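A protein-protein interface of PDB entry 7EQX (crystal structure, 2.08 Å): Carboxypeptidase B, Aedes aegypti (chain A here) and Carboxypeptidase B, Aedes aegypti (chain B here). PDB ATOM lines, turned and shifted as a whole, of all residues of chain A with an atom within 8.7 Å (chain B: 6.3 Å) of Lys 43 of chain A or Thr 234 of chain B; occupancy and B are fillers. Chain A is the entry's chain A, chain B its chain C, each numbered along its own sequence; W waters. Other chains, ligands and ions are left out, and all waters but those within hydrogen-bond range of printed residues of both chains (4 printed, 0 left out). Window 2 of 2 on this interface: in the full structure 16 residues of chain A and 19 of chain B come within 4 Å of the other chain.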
ATOM      1  N   PRO A  17      15.705   7.539   8.185  1.00  0.00           N
ATOM      2  CA  PRO A  17      14.634   6.738   7.581  1.00  0.00           C
ATOM      3  C   PRO A  17      15.027   6.265   6.191  1.00  0.00           C
ATOM      4  O   PRO A  17      15.716   6.966   5.446  1.00  0.00           O
ATOM      5  CB  PRO A  17      13.443   7.703   7.529  1.00  0.00           C
ATOM      6  CG  PRO A  17      13.815   8.855   8.412  1.00  0.00           C
ATOM      7  CD  PRO A  17      15.303   8.939   8.397  1.00  0.00           C
ATOM      8  N   GLU A  18      14.579   5.059   5.845  1.00  0.00           N
ATOM      9  CA  GLU A  18      14.920   4.437   4.572  1.00  0.00           C
ATOM     10  C   GLU A  18      13.762   4.436   3.590  1.00  0.00           C
ATOM     11  O   GLU A  18      13.864   3.817   2.526  1.00  0.00           O
ATOM     12  CB  GLU A  18      15.411   3.009   4.797  1.00  0.00           C
ATOM     13  CG  GLU A  18      16.771   2.951   5.449  1.00  0.00           C
ATOM     14  CD  GLU A  18      17.198   1.544   5.778  1.00  0.00           C
ATOM     15  OE1 GLU A  18      16.810   0.613   5.042  1.00  0.00           O
ATOM     16  OE2 GLU A  18      17.921   1.369   6.777  1.00  0.00           O
ATOM     17  N   SER A  19      12.670   5.111   3.918  1.00  0.00           N
ATOM     18  CA  SER A  19      11.495   5.175   3.064  1.00  0.00           C
ATOM     19  C   SER A  19      10.606   6.303   3.570  1.00  0.00           C
ATOM     20  O   SER A  19      10.745   6.733   4.719  1.00  0.00           O
ATOM     21  CB  SER A  19      10.728   3.842   3.066  1.00  0.00           C
ATOM     22  OG  SER A  19      10.021   3.665   4.281  1.00  0.00           O
ATOM     23  N   PRO A  20       9.699   6.802   2.727  1.00  0.00           N
ATOM     24  CA  PRO A  20       8.718   7.782   3.218  1.00  0.00           C
ATOM     25  C   PRO A  20       7.883   7.272   4.378  1.00  0.00           C
ATOM     26  O   PRO A  20       7.494   8.066   5.245  1.00  0.00           O
ATOM     27  CB  PRO A  20       7.858   8.058   1.978  1.00  0.00           C
ATOM     28  CG  PRO A  20       8.778   7.811   0.830  1.00  0.00           C
ATOM     29  CD  PRO A  20       9.697   6.697   1.257  1.00  0.00           C
ATOM     30  N   ASP A  21       7.588   5.970   4.421  1.00  0.00           N
ATOM     31  CA  ASP A  21       6.806   5.430   5.528  1.00  0.00           C
ATOM     32  C   ASP A  21       7.579   5.495   6.842  1.00  0.00           C
ATOM     33  O   ASP A  21       7.005   5.809   7.890  1.00  0.00           O
ATOM     34  CB  ASP A  21       6.389   3.994   5.222  1.00  0.00           C
ATOM     35  CG  ASP A  21       5.125   3.922   4.391  1.00  0.00           C
ATOM     36  OD1 ASP A  21       4.464   4.968   4.218  1.00  0.00           O
ATOM     37  OD2 ASP A  21       4.791   2.818   3.909  1.00  0.00           O
ATOM     38  N   GLU A  22       8.880   5.200   6.807  1.00  0.00           N
ATOM     39  CA  GLU A  22       9.675   5.273   8.029  1.00  0.00           C
ATOM     40  C   GLU A  22       9.773   6.704   8.540  1.00  0.00           C
ATOM     41  O   GLU A  22       9.675   6.948   9.749  1.00  0.00           O
ATOM     42  CB  GLU A  22      11.071   4.699   7.790  1.00  0.00           C
ATOM     43  CG  GLU A  22      11.107   3.187   7.644  1.00  0.00           C
ATOM     44  CD  GLU A  22      12.501   2.623   7.836  1.00  0.00           C
ATOM     45  OE1 GLU A  22      13.471   3.409   7.820  1.00  0.00           O
ATOM     46  OE2 GLU A  22      12.624   1.394   8.007  1.00  0.00           O
ATOM     47  N   ALA A  23       9.958   7.663   7.630  1.00  0.00           N
ATOM     48  CA  ALA A  23       9.990   9.065   8.027  1.00  0.00           C
ATOM     49  C   ALA A  23       8.659   9.491   8.633  1.00  0.00           C
ATOM     50  O   ALA A  23       8.626  10.253   9.606  1.00  0.00           O
ATOM     51  CB  ALA A  23      10.349   9.942   6.826  1.00  0.00           C
ATOM     52  N   GLU A  24       7.550   9.001   8.073  1.00  0.00           N
ATOM     53  CA  GLU A  24       6.238   9.335   8.611  1.00  0.00           C
ATOM     54  C   GLU A  24       6.061   8.809  10.028  1.00  0.00           C
ATOM     55  O   GLU A  24       5.408   9.462  10.850  1.00  0.00           O
ATOM     56  CB  GLU A  24       5.139   8.786   7.699  1.00  0.00           C
ATOM     57  CG  GLU A  24       3.727   9.041   8.206  1.00  0.00           C
ATOM     58  CD  GLU A  24       2.809   9.576   7.130  1.00  0.00           C
ATOM     59  OE1 GLU A  24       2.182   8.761   6.421  1.00  0.00           O
ATOM     60  OE2 GLU A  24       2.715  10.814   6.992  1.00  0.00           O
ATOM     61  N   TYR A  27       7.425  11.304  12.266  1.00  0.00           N
ATOM     62  CA  TYR A  27       6.528  12.450  12.375  1.00  0.00           C
ATOM     63  C   TYR A  27       5.414  12.198  13.384  1.00  0.00           C
ATOM     64  O   TYR A  27       5.085  13.082  14.184  1.00  0.00           O
ATOM     65  CB  TYR A  27       5.947  12.790  11.004  1.00  0.00           C
ATOM     66  CG  TYR A  27       4.945  13.921  11.027  1.00  0.00           C
ATOM     67  CD1 TYR A  27       5.367  15.242  11.023  1.00  0.00           C
ATOM     68  CD2 TYR A  27       3.580  13.669  11.063  1.00  0.00           C
ATOM     69  CE1 TYR A  27       4.460  16.280  11.049  1.00  0.00           C
ATOM     70  CE2 TYR A  27       2.665  14.702  11.087  1.00  0.00           C
ATOM     71  CZ  TYR A  27       3.110  16.006  11.080  1.00  0.00           C
ATOM     72  OH  TYR A  27       2.203  17.042  11.106  1.00  0.00           O
ATOM     73  N   HIS A  40      15.540  18.054  14.307  1.00  0.00           N
ATOM     74  CA  HIS A  40      15.550  18.053  12.851  1.00  0.00           C
ATOM     75  C   HIS A  40      14.726  16.872  12.355  1.00  0.00           C
ATOM     76  O   HIS A  40      14.895  15.753  12.847  1.00  0.00           O
ATOM     77  CB  HIS A  40      16.993  17.972  12.330  1.00  0.00           C
ATOM     78  CG  HIS A  40      17.118  18.149  10.849  1.00  0.00           C
ATOM     79  ND1 HIS A  40      17.154  19.389  10.248  1.00  0.00           N
ATOM     80  CD2 HIS A  40      17.229  17.242   9.850  1.00  0.00           C
ATOM     81  CE1 HIS A  40      17.274  19.238   8.941  1.00  0.00           C
ATOM     82  NE2 HIS A  40      17.321  17.945   8.673  1.00  0.00           N
ATOM     83  N   LEU A  41      13.839  17.123  11.394  1.00  0.00           N
ATOM     84  CA  LEU A  41      13.026  16.062  10.798  1.00  0.00           C
ATOM     85  C   LEU A  41      12.535  16.540   9.441  1.00  0.00           C
ATOM     86  O   LEU A  41      11.836  17.555   9.363  1.00  0.00           O
ATOM     87  CB  LEU A  41      11.845  15.697  11.698  1.00  0.00           C
ATOM     88  CG  LEU A  41      10.806  14.739  11.103  1.00  0.00           C
ATOM     89  CD1 LEU A  41      11.465  13.482  10.542  1.00  0.00           C
ATOM     90  CD2 LEU A  41       9.744  14.381  12.131  1.00  0.00           C
ATOM     91  N   THR A  42      12.887  15.811   8.380  1.00  0.00           N
ATOM     92  CA  THR A  42      12.477  16.144   7.021  1.00  0.00           C
ATOM     93  C   THR A  42      12.050  14.871   6.298  1.00  0.00           C
ATOM     94  O   THR A  42      12.146  13.762   6.834  1.00  0.00           O
ATOM     95  CB  THR A  42      13.608  16.824   6.232  1.00  0.00           C
ATOM     96  OG1 THR A  42      14.563  15.837   5.831  1.00  0.00           O
ATOM     97  CG2 THR A  42      14.313  17.881   7.066  1.00  0.00           C
ATOM     98  N   LYS A  43      11.557  15.044   5.070  1.00  0.00           N
ATOM     99  CA  LYS A  43      11.288  13.937   4.161  1.00  0.00           C
ATOM    100  C   LYS A  43      12.457  13.649   3.232  1.00  0.00           C
ATOM    101  O   LYS A  43      12.353  12.758   2.382  1.00  0.00           O
ATOM    102  CB  LYS A  43      10.047  14.221   3.306  1.00  0.00           C
ATOM    103  CG  LYS A  43       8.833  14.734   4.052  1.00  0.00           C
ATOM    104  CD  LYS A  43       7.867  15.375   3.067  1.00  0.00           C
ATOM    105  CE  LYS A  43       6.515  15.653   3.695  1.00  0.00           C
ATOM    106  NZ  LYS A  43       5.571  16.240   2.704  1.00  0.00           N
ATOM    107  N   GLN A  44      13.552  14.380   3.369  1.00  0.00           N
ATOM    108  CA  GLN A  44      14.656  14.264   2.429  1.00  0.00           C
ATOM    109  C   GLN A  44      15.299  12.887   2.537  1.00  0.00           C
ATOM    110  O   GLN A  44      15.663  12.461   3.640  1.00  0.00           O
ATOM    111  CB  GLN A  44      15.688  15.356   2.703  1.00  0.00           C
ATOM    112  CG  GLN A  44      16.954  15.253   1.879  1.00  0.00           C
ATOM    113  CD  GLN A  44      17.338  16.575   1.249  1.00  0.00           C
ATOM    114  OE1 GLN A  44      16.604  17.115   0.421  1.00  0.00           O
ATOM    115  NE2 GLN A  44      18.488  17.111   1.644  1.00  0.00           N
ATOM    116  N   PRO A  45      15.447  12.160   1.428  1.00  0.00           N
ATOM    117  CA  PRO A  45      16.086  10.841   1.494  1.00  0.00           C
ATOM    118  C   PRO A  45      17.531  10.956   1.953  1.00  0.00           C
ATOM    119  O   PRO A  45      18.270  11.846   1.524  1.00  0.00           O
ATOM    120  CB  PRO A  45      15.992  10.331   0.051  1.00  0.00           C
ATOM    121  CG  PRO A  45      14.847  11.087  -0.543  1.00  0.00           C
ATOM    122  CD  PRO A  45      14.899  12.446   0.092  1.00  0.00           C
ATOM    123  N   GLY A  46      17.926  10.049   2.845  1.00  0.00           N
ATOM    124  CA  GLY A  46      19.261  10.054   3.399  1.00  0.00           C
ATOM    125  C   GLY A  46      19.498  11.066   4.498  1.00  0.00           C
ATOM    126  O   GLY A  46      20.577  11.052   5.105  1.00  0.00           O
ATOM    127  N   ASP A  47      18.538  11.947   4.769  1.00  0.00           N
ATOM    128  CA  ASP A  47      18.683  12.915   5.846  1.00  0.00           C
ATOM    129  C   ASP A  47      18.586  12.227   7.203  1.00  0.00           C
ATOM    130  O   ASP A  47      17.882  11.227   7.369  1.00  0.00           O
ATOM    131  CB  ASP A  47      17.623  14.009   5.737  1.00  0.00           C
ATOM    132  CG  ASP A  47      17.977  15.247   6.537  1.00  0.00           C
ATOM    133  OD1 ASP A  47      19.167  15.416   6.881  1.00  0.00           O
ATOM    134  OD2 ASP A  47      17.065  16.049   6.829  1.00  0.00           O
ATOM    135  N   GLU A  48      19.306  12.773   8.177  1.00  0.00           N
ATOM    136  CA  GLU A  48      19.328  12.243   9.532  1.00  0.00           C
ATOM    137  C   GLU A  48      18.439  13.095  10.430  1.00  0.00           C
ATOM    138  O   GLU A  48      18.721  14.280  10.647  1.00  0.00           O
ATOM    139  CB  GLU A  48      20.756  12.214  10.072  1.00  0.00           C
ATOM    140  CG  GLU A  48      20.884  11.705  11.498  1.00  0.00           C
ATOM    141  CD  GLU A  48      22.229  11.045  11.757  1.00  0.00           C
ATOM    142  OE1 GLU A  48      23.189  11.343  11.018  1.00  0.00           O
ATOM    143  OE2 GLU A  48      22.330  10.233  12.700  1.00  0.00           O
ATOM    144  N   ALA A  49      17.362  12.501  10.937  1.00  0.00           N
ATOM    145  CA  ALA A  49      16.604  13.135  12.003  1.00  0.00           C
ATOM    146  C   ALA A  49      17.396  13.088  13.305  1.00  0.00           C
ATOM    147  O   ALA A  49      18.132  12.135  13.573  1.00  0.00           O
ATOM    148  CB  ALA A  49      15.252  12.450  12.184  1.00  0.00           C
ATOM    149  N   LEU B 193      13.171  27.166   0.542  1.00  0.00           N
ATOM    150  CA  LEU B 193      11.806  26.678   0.413  1.00  0.00           C
ATOM    151  C   LEU B 193      10.833  27.837   0.246  1.00  0.00           C
ATOM    152  O   LEU B 193      11.101  28.968   0.670  1.00  0.00           O
ATOM    153  CB  LEU B 193      11.406  25.837   1.633  1.00  0.00           C
ATOM    154  CG  LEU B 193      12.370  24.706   2.005  1.00  0.00           C
ATOM    155  CD1 LEU B 193      12.046  24.157   3.380  1.00  0.00           C
ATOM    156  CD2 LEU B 193      12.338  23.600   0.965  1.00  0.00           C
ATOM    157  N   TYR B 194       9.693  27.543  -0.386  1.00  0.00           N
ATOM    158  CA  TYR B 194       8.673  28.554  -0.632  1.00  0.00           C
ATOM    159  C   TYR B 194       7.276  27.963  -0.433  1.00  0.00           C
ATOM    160  O   TYR B 194       7.145  26.742  -0.282  1.00  0.00           O
ATOM    161  CB  TYR B 194       8.855  29.147  -2.034  1.00  0.00           C
ATOM    162  CG  TYR B 194       9.052  28.158  -3.156  1.00  0.00           C
ATOM    163  CD1 TYR B 194       7.963  27.592  -3.810  1.00  0.00           C
ATOM    164  CD2 TYR B 194      10.327  27.817  -3.591  1.00  0.00           C
ATOM    165  CE1 TYR B 194       8.142  26.696  -4.854  1.00  0.00           C
ATOM    166  CE2 TYR B 194      10.512  26.924  -4.632  1.00  0.00           C
ATOM    167  CZ  TYR B 194       9.417  26.367  -5.259  1.00  0.00           C
ATOM    168  OH  TYR B 194       9.598  25.476  -6.295  1.00  0.00           O
ATOM    169  N   TRP B 196       3.474  26.373  -0.762  1.00  0.00           N
ATOM    170  CA  TRP B 196       2.751  26.508   0.505  1.00  0.00           C
ATOM    171  C   TRP B 196       3.332  25.640   1.607  1.00  0.00           C
ATOM    172  O   TRP B 196       3.574  24.448   1.411  1.00  0.00           O
ATOM    173  CB  TRP B 196       1.273  26.147   0.331  1.00  0.00           C
ATOM    174  CG  TRP B 196       0.512  27.027  -0.604  1.00  0.00           C
ATOM    175  CD1 TRP B 196      -0.045  26.664  -1.797  1.00  0.00           C
ATOM    176  CD2 TRP B 196       0.197  28.413  -0.420  1.00  0.00           C
ATOM    177  NE1 TRP B 196      -0.676  27.739  -2.370  1.00  0.00           N
ATOM    178  CE2 TRP B 196      -0.542  28.826  -1.546  1.00  0.00           C
ATOM    179  CE3 TRP B 196       0.474  29.348   0.587  1.00  0.00           C
ATOM    180  CZ2 TRP B 196      -1.011  30.131  -1.696  1.00  0.00           C
ATOM    181  CZ3 TRP B 196       0.007  30.648   0.434  1.00  0.00           C
ATOM    182  CH2 TRP B 196      -0.729  31.025  -0.698  1.00  0.00           C
ATOM    183  N   GLY B 197       3.543  26.237   2.779  1.00  0.00           N
ATOM    184  CA  GLY B 197       3.894  25.439   3.938  1.00  0.00           C
ATOM    185  C   GLY B 197       2.768  24.530   4.389  1.00  0.00           C
ATOM    186  O   GLY B 197       3.015  23.412   4.851  1.00  0.00           O
ATOM    187  N   TRP B 198       1.521  24.983   4.247  1.00  0.00           N
ATOM    188  CA  TRP B 198       0.378  24.286   4.821  1.00  0.00           C
ATOM    189  C   TRP B 198      -0.231  23.227   3.907  1.00  0.00           C
ATOM    190  O   TRP B 198      -1.045  22.426   4.382  1.00  0.00           O
ATOM    191  CB  TRP B 198      -0.705  25.298   5.220  1.00  0.00           C
ATOM    192  CG  TRP B 198      -1.533  25.809   4.076  1.00  0.00           C
ATOM    193  CD1 TRP B 198      -1.250  26.872   3.266  1.00  0.00           C
ATOM    194  CD2 TRP B 198      -2.790  25.288   3.630  1.00  0.00           C
ATOM    195  NE1 TRP B 198      -2.251  27.040   2.337  1.00  0.00           N
ATOM    196  CE2 TRP B 198      -3.208  26.080   2.539  1.00  0.00           C
ATOM    197  CE3 TRP B 198      -3.602  24.229   4.045  1.00  0.00           C
ATOM    198  CZ2 TRP B 198      -4.399  25.841   1.859  1.00  0.00           C
ATOM    199  CZ3 TRP B 198      -4.785  23.994   3.367  1.00  0.00           C
ATOM    200  CH2 TRP B 198      -5.171  24.796   2.286  1.00  0.00           C
ATOM    201  N   THR B 199       0.130  23.187   2.626  1.00  0.00           N
ATOM    202  CA  THR B 199      -0.451  22.193   1.733  1.00  0.00           C
ATOM    203  C   THR B 199       0.537  21.858   0.624  1.00  0.00           C
ATOM    204  O   THR B 199       1.408  22.659   0.273  1.00  0.00           O
ATOM    205  CB  THR B 199      -1.782  22.670   1.131  1.00  0.00           C
ATOM    206  OG1 THR B 199      -2.280  21.675   0.229  1.00  0.00           O
ATOM    207  CG2 THR B 199      -1.596  23.969   0.365  1.00  0.00           C
ATOM    208  N   SER B 200       0.367  20.659   0.057  1.00  0.00           N
ATOM    209  CA  SER B 200       1.224  20.184  -1.023  1.00  0.00           C
ATOM    210  C   SER B 200       0.828  20.739  -2.387  1.00  0.00           C
ATOM    211  O   SER B 200       1.627  20.655  -3.327  1.00  0.00           O
ATOM    212  CB  SER B 200       1.219  18.655  -1.066  1.00  0.00           C
ATOM    213  OG  SER B 200       0.078  18.174  -1.750  1.00  0.00           O
ATOM    214  N   LYS B 201      -0.378  21.288  -2.523  1.00  0.00           N
ATOM    215  CA  LYS B 201      -0.807  21.846  -3.799  1.00  0.00           C
ATOM    216  C   LYS B 201       0.053  23.057  -4.138  1.00  0.00           C
ATOM    217  O   LYS B 201       0.209  23.969  -3.319  1.00  0.00           O
ATOM    218  CB  LYS B 201      -2.284  22.236  -3.732  1.00  0.00           C
ATOM    219  CG  LYS B 201      -2.844  22.932  -4.976  1.00  0.00           C
ATOM    220  CD  LYS B 201      -2.473  22.196  -6.252  1.00  0.00           C
ATOM    221  CE  LYS B 201      -3.661  22.040  -7.188  1.00  0.00           C
ATOM    222  NZ  LYS B 201      -3.466  20.882  -8.107  1.00  0.00           N
ATOM    223  N   GLY B 231      12.780  23.875  -3.267  1.00  0.00           N
ATOM    224  CA  GLY B 231      11.458  23.453  -3.679  1.00  0.00           C
ATOM    225  C   GLY B 231      10.386  24.051  -2.796  1.00  0.00           C
ATOM    226  O   GLY B 231      10.662  24.790  -1.847  1.00  0.00           O
ATOM    227  N   SER B 232       9.146  23.708  -3.135  1.00  0.00           N
ATOM    228  CA  SER B 232       8.025  24.017  -2.262  1.00  0.00           C
ATOM    229  C   SER B 232       8.199  23.292  -0.933  1.00  0.00           C
ATOM    230  O   SER B 232       8.752  22.190  -0.877  1.00  0.00           O
ATOM    231  CB  SER B 232       6.710  23.607  -2.924  1.00  0.00           C
ATOM    232  OG  SER B 232       5.612  24.305  -2.363  1.00  0.00           O
ATOM    233  N   SER B 233       7.719  23.926   0.142  1.00  0.00           N
ATOM    234  CA  SER B 233       8.032  23.475   1.498  1.00  0.00           C
ATOM    235  C   SER B 233       7.741  21.993   1.699  1.00  0.00           C
ATOM    236  O   SER B 233       8.581  21.251   2.221  1.00  0.00           O
ATOM    237  CB  SER B 233       7.247  24.302   2.521  1.00  0.00           C
ATOM    238  OG  SER B 233       7.897  25.528   2.789  1.00  0.00           O
ATOM    239  N   THR B 234       6.554  21.540   1.286  1.00  0.00           N
ATOM    240  CA  THR B 234       6.146  20.165   1.557  1.00  0.00           C
ATOM    241  C   THR B 234       6.976  19.130   0.805  1.00  0.00           C
ATOM    242  O   THR B 234       6.881  17.941   1.131  1.00  0.00           O
ATOM    243  CB  THR B 234       4.661  19.976   1.240  1.00  0.00           C
ATOM    244  OG1 THR B 234       4.417  20.282  -0.137  1.00  0.00           O
ATOM    245  CG2 THR B 234       3.814  20.892   2.121  1.00  0.00           C
ATOM    246  N   ASN B 235       7.767  19.542  -0.191  1.00  0.00           N
ATOM    247  CA  ASN B 235       8.753  18.628  -0.765  1.00  0.00           C
ATOM    248  C   ASN B 235       9.713  18.115   0.299  1.00  0.00           C
ATOM    249  O   ASN B 235      10.163  16.965   0.231  1.00  0.00           O
ATOM    250  CB  ASN B 235       9.551  19.315  -1.878  1.00  0.00           C
ATOM    251  CG  ASN B 235       8.745  19.513  -3.144  1.00  0.00           C
ATOM    252  OD1 ASN B 235       7.534  19.291  -3.168  1.00  0.00           O
ATOM    253  ND2 ASN B 235       9.417  19.932  -4.210  1.00  0.00           N
ATOM    254  N   VAL B 236      10.040  18.953   1.285  1.00  0.00           N
ATOM    255  CA  VAL B 236      11.076  18.660   2.262  1.00  0.00           C
ATOM    256  C   VAL B 236      10.509  18.517   3.669  1.00  0.00           C
ATOM    257  O   VAL B 236      10.888  17.598   4.404  1.00  0.00           O
ATOM    258  CB  VAL B 236      12.177  19.742   2.229  1.00  0.00           C
ATOM    259  CG1 VAL B 236      13.184  19.525   3.348  1.00  0.00           C
ATOM    260  CG2 VAL B 236      12.866  19.748   0.876  1.00  0.00           C
ATOM    261  N   LEU B 237       9.595  19.401   4.059  1.00  0.00           N
ATOM    262  CA  LEU B 237       9.056  19.437   5.409  1.00  0.00           C
ATOM    263  C   LEU B 237       7.596  19.007   5.410  1.00  0.00           C
ATOM    264  O   LEU B 237       6.862  19.240   4.448  1.00  0.00           O
ATOM    265  CB  LEU B 237       9.171  20.842   6.006  1.00  0.00           C
ATOM    266  CG  LEU B 237      10.550  21.499   5.952  1.00  0.00           C
ATOM    267  CD1 LEU B 237      10.474  22.932   6.462  1.00  0.00           C
ATOM    268  CD2 LEU B 237      11.555  20.690   6.755  1.00  0.00           C
ATOM    269  N   TYR B 238       7.176  18.389   6.507  1.00  0.00           N
ATOM    270  CA  TYR B 238       5.774  18.039   6.659  1.00  0.00           C
ATOM    271  C   TYR B 238       4.928  19.303   6.768  1.00  0.00           C
ATOM    272  O   TYR B 238       5.360  20.319   7.318  1.00  0.00           O
ATOM    273  CB  TYR B 238       5.585  17.142   7.879  1.00  0.00           C
ATOM    274  CG  TYR B 238       6.216  15.785   7.682  1.00  0.00           C
ATOM    275  CD1 TYR B 238       5.543  14.780   6.998  1.00  0.00           C
ATOM    276  CD2 TYR B 238       7.498  15.519   8.146  1.00  0.00           C
ATOM    277  CE1 TYR B 238       6.121  13.542   6.798  1.00  0.00           C
ATOM    278  CE2 TYR B 238       8.086  14.282   7.951  1.00  0.00           C
ATOM    279  CZ  TYR B 238       7.392  13.298   7.276  1.00  0.00           C
ATOM    280  OH  TYR B 238       7.970  12.065   7.078  1.00  0.00           O
ATOM    281  N   ALA B 239       3.716  19.228   6.223  1.00  0.00           N
ATOM    282  CA  ALA B 239       2.853  20.398   6.126  1.00  0.00           C
ATOM    283  C   ALA B 239       2.596  21.012   7.496  1.00  0.00           C
ATOM    284  O   ALA B 239       2.352  20.307   8.479  1.00  0.00           O
ATOM    285  CB  ALA B 239       1.529  20.022   5.461  1.00  0.00           C
ATOM    286  N   ALA B 240       2.674  22.338   7.555  1.00  0.00           N
ATOM    287  CA  ALA B 240       2.420  23.081   8.783  1.00  0.00           C
ATOM    288  C   ALA B 240       1.794  24.419   8.419  1.00  0.00           C
ATOM    289  O   ALA B 240       2.275  25.107   7.514  1.00  0.00           O
ATOM    290  CB  ALA B 240       3.708  23.291   9.587  1.00  0.00           C
HETATM  291  O   HOH W   1       9.187  18.627   8.618  1.00  0.00           O
HETATM  292  O   HOH W   2       3.252  16.772   4.393  1.00  0.00           O
HETATM  293  O   HOH W   3       1.455  17.639   8.233  1.00  0.00           O
HETATM  294  O   HOH W   4       7.014  10.668   5.016  1.00  0.00           O
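The backbone NH of Gln 44 of chain A sits at hydrogen-bond distance from the side-chain hydroxyl of Thr 42 of chain A (3.0 Å).
The side-chain hydroxyl of Thr 42 of chain A sits at hydrogen-bond distance from the side-chain carboxylate of Asp 47 of chain A (2.7 Å).
Printed residues of chain B within 4 Å of Lys 43 of chain A: Thr 234 (2.7 Å), Asn 235 (3.98 Å), Val 236 (2.7 Å), Leu 237 (3.7 Å) and Tyr 238 (3.6 Å).
Thr 234 of chain B touches one residue of chain A.
No residue of chain A comes within 4 Å of Ser 233 of chain B.
Printed residues of chain B within 4 Å of Glu 24 of chain A: Tyr 238.
Printed residues of chain A within 4 Å of Asn 235 of chain B: Lys 43.
Of the printed residues of chain B, Ala 23 of chain A touches Tyr 238.
Of the printed residues of chain A, Val 236 of chain B touches Thr 42 and Lys 43.
The nearest printed residue of chain B that does not touch Lys 43 of chain A is Ala 239 of chain B (5.0 Å).
The nearest printed residue of chain B that does not touch Glu 24 of chain A is Ala 239 of chain B (8.5 Å).
Among the printed residues, pairs that only touch across the chains: Tyr 27 of chain A with Tyr 238 of chain B, Thr 42 of chain A with Val 236 of chain B, Thr 42 of chain A with Leu 237 of chain B, Lys 43 of chain A with Asn 235 of chain B, Lys 43 of chain A with Leu 237 of chain B and Lys 43 of chain A with Tyr 238 of chain B.
The backbone carbonyl oxygen (O) of Ala 23 of chain A lies close to the side-chain hydroxyl (OH) of Tyr 238 of chain B, at 3.2 Å.
The side-chain hydroxyl of Tyr 238 of chain B sits at hydrogen-bond distance from the backbone NH of Glu 24 of chain A, 3.2 Å away.
NZ of Lys 43 of chain A lies within hydrogen-bond range of O of Thr 234 of chain B (2.7 Å).
N of Lys 43 of chain A is in hydrogen-bond range of O of Val 236 of chain B, at 2.7 Å.
Of the 19 printed residues of chain A, 5 touch a printed residue of chain B.
Among the printed residues, 10 pairs touch across the chains.
Among the printed residues, no Asp or Glu carboxylate lies within 4 Å of a Lys or Arg side-chain nitrogen of the other chain.
Water W4 bridges the backbone carbonyl oxygen (O) of Pro 20 of chain A and the side-chain hydroxyl (OH) of Tyr 238 of chain B.
Water W3 lies within hydrogen-bond range of the backbone carbonyl oxygen (O) of Ala 239 of chain B (2.8 Å) and the side-chain hydroxyl (OH) of Tyr 27 of chain A (3.0 Å).
Water W2 lies within hydrogen-bond range of NZ of Lys 43 of chain A (2.9 Å) and N of Ala 239 of chain B (3.1 Å).
Water W1 bridges the backbone NH of Tyr 238 of chain B (2.9 Å) and the backbone carbonyl oxygen of Leu 41 of chain A (3.0 Å).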
